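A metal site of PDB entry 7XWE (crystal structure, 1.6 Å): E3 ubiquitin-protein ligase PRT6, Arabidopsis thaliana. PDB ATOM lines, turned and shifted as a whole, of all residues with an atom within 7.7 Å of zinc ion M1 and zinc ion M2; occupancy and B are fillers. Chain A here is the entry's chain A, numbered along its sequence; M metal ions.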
ATOM      1  N   SER A   4      32.666 -10.147 -21.472  1.00  0.00           N
ATOM      2  CA  SER A   4      31.408 -10.263 -22.199  1.00  0.00           C
ATOM      3  C   SER A   4      31.415  -9.293 -23.368  1.00  0.00           C
ATOM      4  O   SER A   4      32.247  -8.380 -23.459  1.00  0.00           O
ATOM      5  CB  SER A   4      30.197 -10.003 -21.292  1.00  0.00           C
ATOM      6  OG  SER A   4      29.026 -10.597 -21.852  1.00  0.00           O
ATOM      7  N   GLY A   7      30.168 -10.741 -29.004  1.00  0.00           N
ATOM      8  CA  GLY A   7      29.408 -11.896 -29.448  1.00  0.00           C
ATOM      9  C   GLY A   7      29.492 -13.074 -28.522  1.00  0.00           C
ATOM     10  O   GLY A   7      29.408 -14.220 -28.977  1.00  0.00           O
ATOM     11  N   VAL A   8      29.686 -12.834 -27.234  1.00  0.00           N
ATOM     12  CA  VAL A   8      29.845 -13.882 -26.235  1.00  0.00           C
ATOM     13  C   VAL A   8      29.273 -13.346 -24.935  1.00  0.00           C
ATOM     14  O   VAL A   8      29.494 -12.182 -24.587  1.00  0.00           O
ATOM     15  CB  VAL A   8      31.326 -14.274 -26.057  1.00  0.00           C
ATOM     16  CG1 VAL A   8      32.127 -13.073 -25.576  1.00  0.00           C
ATOM     17  CG2 VAL A   8      31.460 -15.426 -25.089  1.00  0.00           C
ATOM     18  N   CYS A   9      28.553 -14.195 -24.201  1.00  0.00           N
ATOM     19  CA  CYS A   9      27.980 -13.766 -22.932  1.00  0.00           C
ATOM     20  C   CYS A   9      28.997 -13.816 -21.803  1.00  0.00           C
ATOM     21  O   CYS A   9      29.249 -12.815 -21.128  1.00  0.00           O
ATOM     22  CB  CYS A   9      26.764 -14.609 -22.579  1.00  0.00           C
ATOM     23  SG  CYS A   9      26.046 -14.187 -20.959  1.00  0.00           S
ATOM     24  N   GLY A  10      29.520 -15.002 -21.514  1.00  0.00           N
ATOM     25  CA  GLY A  10      30.510 -15.188 -20.470  1.00  0.00           C
ATOM     26  C   GLY A  10      30.053 -15.043 -19.026  1.00  0.00           C
ATOM     27  O   GLY A  10      30.895 -15.210 -18.135  1.00  0.00           O
ATOM     28  N   SER A  11      28.789 -14.715 -18.762  1.00  0.00           N
ATOM     29  CA  SER A  11      28.308 -14.621 -17.383  1.00  0.00           C
ATOM     30  C   SER A  11      28.812 -15.795 -16.549  1.00  0.00           C
ATOM     31  O   SER A  11      28.730 -16.950 -16.984  1.00  0.00           O
ATOM     32  CB  SER A  11      26.783 -14.583 -17.330  1.00  0.00           C
ATOM     33  OG  SER A  11      26.278 -13.279 -17.486  1.00  0.00           O
ATOM     34  N   VAL A  12      29.317 -15.510 -15.351  1.00  0.00           N
ATOM     35  CA  VAL A  12      29.930 -16.523 -14.488  1.00  0.00           C
ATOM     36  C   VAL A  12      28.989 -16.815 -13.327  1.00  0.00           C
ATOM     37  O   VAL A  12      28.477 -15.883 -12.688  1.00  0.00           O
ATOM     38  CB  VAL A  12      31.306 -16.091 -13.975  1.00  0.00           C
ATOM     39  CG1 VAL A  12      31.789 -17.027 -12.862  1.00  0.00           C
ATOM     40  CG2 VAL A  12      32.317 -16.021 -15.110  1.00  0.00           C
ATOM     41  N   TRP A  13      28.777 -18.091 -13.048  1.00  0.00           N
ATOM     42  CA  TRP A  13      27.859 -18.524 -12.000  1.00  0.00           C
ATOM     43  C   TRP A  13      28.594 -18.885 -10.705  1.00  0.00           C
ATOM     44  O   TRP A  13      29.727 -19.365 -10.732  1.00  0.00           O
ATOM     45  CB  TRP A  13      27.056 -19.756 -12.436  1.00  0.00           C
ATOM     46  CG  TRP A  13      26.149 -19.529 -13.599  1.00  0.00           C
ATOM     47  CD1 TRP A  13      25.166 -18.608 -13.715  1.00  0.00           C
ATOM     48  CD2 TRP A  13      26.162 -20.260 -14.840  1.00  0.00           C
ATOM     49  NE1 TRP A  13      24.556 -18.709 -14.954  1.00  0.00           N
ATOM     50  CE2 TRP A  13      25.155 -19.716 -15.658  1.00  0.00           C
ATOM     51  CE3 TRP A  13      26.932 -21.324 -15.332  1.00  0.00           C
ATOM     52  CZ2 TRP A  13      24.890 -20.206 -16.936  1.00  0.00           C
ATOM     53  CZ3 TRP A  13      26.673 -21.804 -16.601  1.00  0.00           C
ATOM     54  CH2 TRP A  13      25.653 -21.239 -17.388  1.00  0.00           C
ATOM     55  N   ALA A  32      25.363 -24.968 -20.861  1.00  0.00           N
ATOM     56  CA  ALA A  32      24.205 -24.310 -20.250  1.00  0.00           C
ATOM     57  C   ALA A  32      24.226 -22.845 -20.622  1.00  0.00           C
ATOM     58  O   ALA A  32      25.272 -22.300 -20.975  1.00  0.00           O
ATOM     59  CB  ALA A  32      24.206 -24.466 -18.728  1.00  0.00           C
ATOM     60  N   ILE A  33      23.065 -22.206 -20.522  1.00  0.00           N
ATOM     61  CA  ILE A  33      23.012 -20.756 -20.762  1.00  0.00           C
ATOM     62  C   ILE A  33      22.261 -20.087 -19.628  1.00  0.00           C
ATOM     63  O   ILE A  33      21.374 -20.679 -18.996  1.00  0.00           O
ATOM     64  CB  ILE A  33      22.381 -20.367 -22.120  1.00  0.00           C
ATOM     65  CG1 ILE A  33      20.944 -20.872 -22.253  1.00  0.00           C
ATOM     66  CG2 ILE A  33      23.277 -20.889 -23.292  1.00  0.00           C
ATOM     67  CD1 ILE A  33      20.223 -20.275 -23.483  1.00  0.00           C
ATOM     68  N   CYS A  34      22.605 -18.831 -19.390  1.00  0.00           N
ATOM     69  CA  CYS A  34      22.035 -18.095 -18.275  1.00  0.00           C
ATOM     70  C   CYS A  34      20.564 -17.749 -18.545  1.00  0.00           C
ATOM     71  O   CYS A  34      20.086 -17.774 -19.689  1.00  0.00           O
ATOM     72  CB  CYS A  34      22.870 -16.849 -18.001  1.00  0.00           C
ATOM     73  SG  CYS A  34      22.735 -15.523 -19.214  1.00  0.00           S
ATOM     74  N   VAL A  35      19.830 -17.476 -17.470  1.00  0.00           N
ATOM     75  CA  VAL A  35      18.394 -17.235 -17.605  1.00  0.00           C
ATOM     76  C   VAL A  35      18.087 -16.076 -18.549  1.00  0.00           C
ATOM     77  O   VAL A  35      17.214 -16.222 -19.410  1.00  0.00           O
ATOM     78  CB  VAL A  35      17.760 -17.035 -16.208  1.00  0.00           C
ATOM     79  CG1 VAL A  35      16.300 -16.666 -16.374  1.00  0.00           C
ATOM     80  CG2 VAL A  35      17.878 -18.345 -15.422  1.00  0.00           C
ATOM     81  N   PRO A  36      18.776 -14.924 -18.466  1.00  0.00           N
ATOM     82  CA  PRO A  36      18.501 -13.847 -19.457  1.00  0.00           C
ATOM     83  C   PRO A  36      18.733 -14.271 -20.887  1.00  0.00           C
ATOM     84  O   PRO A  36      17.941 -13.931 -21.757  1.00  0.00           O
ATOM     85  CB  PRO A  36      19.490 -12.742 -19.048  1.00  0.00           C
ATOM     86  CG  PRO A  36      19.778 -12.995 -17.595  1.00  0.00           C
ATOM     87  CD  PRO A  36      19.697 -14.480 -17.401  1.00  0.00           C
ATOM     88  N   CYS A  37      19.826 -14.982 -21.172  1.00  0.00           N
ATOM     89  CA  CYS A  37      20.040 -15.406 -22.545  1.00  0.00           C
ATOM     90  C   CYS A  37      18.977 -16.391 -22.988  1.00  0.00           C
ATOM     91  O   CYS A  37      18.511 -16.369 -24.146  1.00  0.00           O
ATOM     92  CB  CYS A  37      21.410 -16.081 -22.672  1.00  0.00           C
ATOM     93  SG  CYS A  37      22.846 -14.941 -22.543  1.00  0.00           S
ATOM     94  N   PHE A  38      18.536 -17.321 -22.107  1.00  0.00           N
ATOM     95  CA  PHE A  38      17.442 -18.216 -22.459  1.00  0.00           C
ATOM     96  C   PHE A  38      16.196 -17.417 -22.796  1.00  0.00           C
ATOM     97  O   PHE A  38      15.537 -17.676 -23.809  1.00  0.00           O
ATOM     98  CB  PHE A  38      17.137 -19.186 -21.314  1.00  0.00           C
ATOM     99  CG  PHE A  38      16.027 -20.147 -21.640  1.00  0.00           C
ATOM    100  CD1 PHE A  38      16.299 -21.303 -22.371  1.00  0.00           C
ATOM    101  CD2 PHE A  38      14.744 -19.873 -21.271  1.00  0.00           C
ATOM    102  CE1 PHE A  38      15.294 -22.181 -22.696  1.00  0.00           C
ATOM    103  CE2 PHE A  38      13.736 -20.748 -21.574  1.00  0.00           C
ATOM    104  CZ  PHE A  38      14.008 -21.905 -22.305  1.00  0.00           C
ATOM    105  N   ASN A  40      15.913 -14.415 -23.854  1.00  0.00           N
ATOM    106  CA  ASN A  40      16.068 -13.606 -25.057  1.00  0.00           C
ATOM    107  C   ASN A  40      16.366 -14.441 -26.311  1.00  0.00           C
ATOM    108  O   ASN A  40      16.745 -13.885 -27.351  1.00  0.00           O
ATOM    109  CB  ASN A  40      17.147 -12.560 -24.826  1.00  0.00           C
ATOM    110  CG  ASN A  40      16.710 -11.458 -23.873  1.00  0.00           C
ATOM    111  OD1 ASN A  40      17.404 -11.121 -22.910  1.00  0.00           O
ATOM    112  ND2 ASN A  40      15.582 -10.845 -24.176  1.00  0.00           N
ATOM    113  N   GLY A  41      16.132 -15.762 -26.254  1.00  0.00           N
ATOM    114  CA  GLY A  41      16.306 -16.616 -27.408  1.00  0.00           C
ATOM    115  C   GLY A  41      15.029 -17.389 -27.740  1.00  0.00           C
ATOM    116  O   GLY A  41      13.977 -17.185 -27.137  1.00  0.00           O
ATOM    117  N   CYS A  57      30.206 -20.977 -16.584  1.00  0.00           N
ATOM    118  CA  CYS A  57      29.890 -19.760 -17.291  1.00  0.00           C
ATOM    119  C   CYS A  57      28.943 -20.062 -18.435  1.00  0.00           C
ATOM    120  O   CYS A  57      28.894 -21.174 -18.963  1.00  0.00           O
ATOM    121  CB  CYS A  57      31.167 -19.080 -17.802  1.00  0.00           C
ATOM    122  SG  CYS A  57      31.952 -19.909 -19.160  1.00  0.00           S
ATOM    123  N   CYS A  58      28.161 -19.040 -18.801  1.00  0.00           N
ATOM    124  CA  CYS A  58      27.171 -19.178 -19.858  1.00  0.00           C
ATOM    125  C   CYS A  58      27.821 -19.448 -21.200  1.00  0.00           C
ATOM    126  O   CYS A  58      28.822 -18.829 -21.559  1.00  0.00           O
ATOM    127  CB  CYS A  58      26.344 -17.889 -19.949  1.00  0.00           C
ATOM    128  SG  CYS A  58      25.137 -17.825 -21.233  1.00  0.00           S
ATOM    129  N   ASP A  59      27.221 -20.355 -21.959  1.00  0.00           N
ATOM    130  CA  ASP A  59      27.765 -20.738 -23.258  1.00  0.00           C
ATOM    131  C   ASP A  59      27.176 -19.966 -24.421  1.00  0.00           C
ATOM    132  O   ASP A  59      27.562 -20.220 -25.555  1.00  0.00           O
ATOM    133  CB  ASP A  59      27.556 -22.241 -23.464  1.00  0.00           C
ATOM    134  CG  ASP A  59      28.379 -23.061 -22.501  1.00  0.00           C
ATOM    135  OD1 ASP A  59      29.571 -22.753 -22.327  1.00  0.00           O
ATOM    136  OD2 ASP A  59      27.818 -23.982 -21.893  1.00  0.00           O
ATOM    137  N   CYS A  60      26.252 -19.041 -24.169  1.00  0.00           N
ATOM    138  CA  CYS A  60      25.597 -18.290 -25.245  1.00  0.00           C
ATOM    139  C   CYS A  60      26.603 -17.491 -26.041  1.00  0.00           C
ATOM    140  O   CYS A  60      27.423 -16.766 -25.488  1.00  0.00           O
ATOM    141  CB  CYS A  60      24.545 -17.366 -24.626  1.00  0.00           C
ATOM    142  SG  CYS A  60      23.563 -16.532 -25.922  1.00  0.00           S
ATOM    143  N   GLY A  61      26.522 -17.629 -27.374  1.00  0.00           N
ATOM    144  CA  GLY A  61      27.440 -16.992 -28.291  1.00  0.00           C
ATOM    145  C   GLY A  61      28.688 -17.785 -28.633  1.00  0.00           C
ATOM    146  O   GLY A  61      29.461 -17.346 -29.491  1.00  0.00           O
ATOM    147  N   GLY A  70      20.317 -21.230 -31.267  1.00  0.00           N
ATOM    148  CA  GLY A  70      19.968 -21.088 -29.876  1.00  0.00           C
ATOM    149  C   GLY A  70      20.616 -19.921 -29.169  1.00  0.00           C
ATOM    150  O   GLY A  70      20.430 -19.779 -27.952  1.00  0.00           O
ATOM    151  N   PHE A  71      21.384 -19.107 -29.885  1.00  0.00           N
ATOM    152  CA  PHE A  71      21.940 -17.878 -29.323  1.00  0.00           C
ATOM    153  C   PHE A  71      20.801 -16.904 -29.043  1.00  0.00           C
ATOM    154  O   PHE A  71      19.819 -16.851 -29.777  1.00  0.00           O
ATOM    155  CB  PHE A  71      22.917 -17.212 -30.297  1.00  0.00           C
ATOM    156  CG  PHE A  71      24.231 -17.958 -30.515  1.00  0.00           C
ATOM    157  CD1 PHE A  71      25.095 -17.521 -31.500  1.00  0.00           C
ATOM    158  CD2 PHE A  71      24.598 -19.062 -29.761  1.00  0.00           C
ATOM    159  CE1 PHE A  71      26.291 -18.179 -31.737  1.00  0.00           C
ATOM    160  CE2 PHE A  71      25.800 -19.708 -30.003  1.00  0.00           C
ATOM    161  CZ  PHE A  71      26.649 -19.265 -30.973  1.00  0.00           C
ATOM    162  N   CYS A  72      20.947 -16.119 -27.974  1.00  0.00           N
ATOM    163  CA  CYS A  72      19.985 -15.076 -27.678  1.00  0.00           C
ATOM    164  C   CYS A  72      20.177 -13.907 -28.646  1.00  0.00           C
ATOM    165  O   CYS A  72      21.165 -13.831 -29.388  1.00  0.00           O
ATOM    166  CB  CYS A  72      20.129 -14.606 -26.221  1.00  0.00           C
ATOM    167  SG  CYS A  72      21.431 -13.389 -25.920  1.00  0.00           S
ATOM    168  N   SER A  73      19.222 -12.983 -28.625  1.00  0.00           N
ATOM    169  CA  SER A  73      19.218 -11.873 -29.574  1.00  0.00           C
ATOM    170  C   SER A  73      20.415 -10.944 -29.406  1.00  0.00           C
ATOM    171  O   SER A  73      20.741 -10.184 -30.325  1.00  0.00           O
ATOM    172  CB  SER A  73      17.924 -11.086 -29.413  1.00  0.00           C
ATOM    173  OG  SER A  73      17.910 -10.480 -28.127  1.00  0.00           O
ATOM    174  N   ASN A  74      21.086 -10.999 -28.254  1.00  0.00           N
ATOM    175  CA  ASN A  74      22.185 -10.081 -27.941  1.00  0.00           C
ATOM    176  C   ASN A  74      23.578 -10.670 -28.154  1.00  0.00           C
ATOM    177  O   ASN A  74      24.559  -9.924 -28.057  1.00  0.00           O
ATOM    178  CB  ASN A  74      22.061  -9.606 -26.500  1.00  0.00           C
ATOM    179  CG  ASN A  74      20.797  -8.831 -26.254  1.00  0.00           C
ATOM    180  OD1 ASN A  74      20.022  -9.137 -25.332  1.00  0.00           O
ATOM    181  ND2 ASN A  74      20.560  -7.845 -27.079  1.00  0.00           N
ATOM    182  N   HIS A  75      23.711 -11.970 -28.389  1.00  0.00           N
ATOM    183  CA  HIS A  75      25.017 -12.586 -28.595  1.00  0.00           C
ATOM    184  C   HIS A  75      25.076 -13.270 -29.963  1.00  0.00           C
ATOM    185  O   HIS A  75      25.745 -14.308 -30.133  1.00  0.00           O
ATOM    186  CB  HIS A  75      25.345 -13.533 -27.439  1.00  0.00           C
ATOM    187  CG  HIS A  75      25.392 -12.831 -26.114  1.00  0.00           C
ATOM    188  ND1 HIS A  75      24.549 -13.140 -25.067  1.00  0.00           N
ATOM    189  CD2 HIS A  75      26.151 -11.786 -25.687  1.00  0.00           C
ATOM    190  CE1 HIS A  75      24.794 -12.338 -24.057  1.00  0.00           C
ATOM    191  NE2 HIS A  75      25.762 -11.515 -24.400  1.00  0.00           N
ATOM    192  N   LYS A  76      24.372 -12.656 -30.903  1.00  0.00           N
ATOM    193  CA  LYS A  76      24.262 -12.945 -32.339  1.00  0.00           C
ATOM    194  C   LYS A  76      23.396 -14.152 -32.601  1.00  0.00           C
ATOM    195  O   LYS A  76      22.190 -13.976 -32.824  1.00  0.00           O
ATOM    196  CB  LYS A  76      25.637 -13.074 -32.969  1.00  0.00           C
ATOM    197  CG  LYS A  76      26.445 -11.820 -32.687  1.00  0.00           C
ATOM    198  CD  LYS A  76      27.435 -11.504 -33.779  1.00  0.00           C
ATOM    199  CE  LYS A  76      28.832 -11.992 -33.433  1.00  0.00           C
ATOM    200  NZ  LYS A  76      29.826 -10.918 -33.780  1.00  0.00           N
HETATM  201 ZN    ZN M   1      24.296 -15.686 -20.917  1.00  0.00          ZN
HETATM  202 ZN    ZN M   2      23.136 -14.572 -24.938  1.00  0.00          ZN
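Of the 29 residues printed, 4 come within 4 Å of zinc ion M2.
N of Cys 9 is in hydrogen-bond range of O of Cys 60.
N of Cys 60 lies close to SG of Cys 58 (3.4 Å).
SG of Cys 72 sits close to N of Asn 74 (3.4 Å).
The side-chain sulfur of Cys 9 sits close to the backbone NH of Ser 11 (3.6 Å).
The backbone NH (N) of Cys 58 is in hydrogen-bond range of the backbone carbonyl oxygen (O) of Ser 11, 2.8 Å away.
Zinc ion M1 is bound by SG of Cys 37.
The side-chain sulfur (SG) of Cys 9 is bound to zinc ion M1, 2.3 Å away.
The side-chain sulfur (SG) of Cys 34 binds zinc ion M1 (2.3 Å).
SG of Cys 58 is bound to zinc ion M1 (2.3 Å).
Zinc ion M1 has four donor atoms within binding distance.
ND1 of His 75 is bound to zinc ion M2, 2.0 Å away.
Zinc ion M2 is bound by SG of Cys 60, at 2.2 Å.
The side-chain sulfur (SG) of Cys 72 is bound to zinc ion M2, at 2.3 Å.
SG of Cys 37 is bound to zinc ion M2, 2.4 Å away.
Four residues have an atom within 4 Å of zinc ion M1: Cys 9, Cys 34, Cys 37 and Cys 58.
The nearest printed residue that does not touch zinc ion M1 is Cys 60 (4.1 Å).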
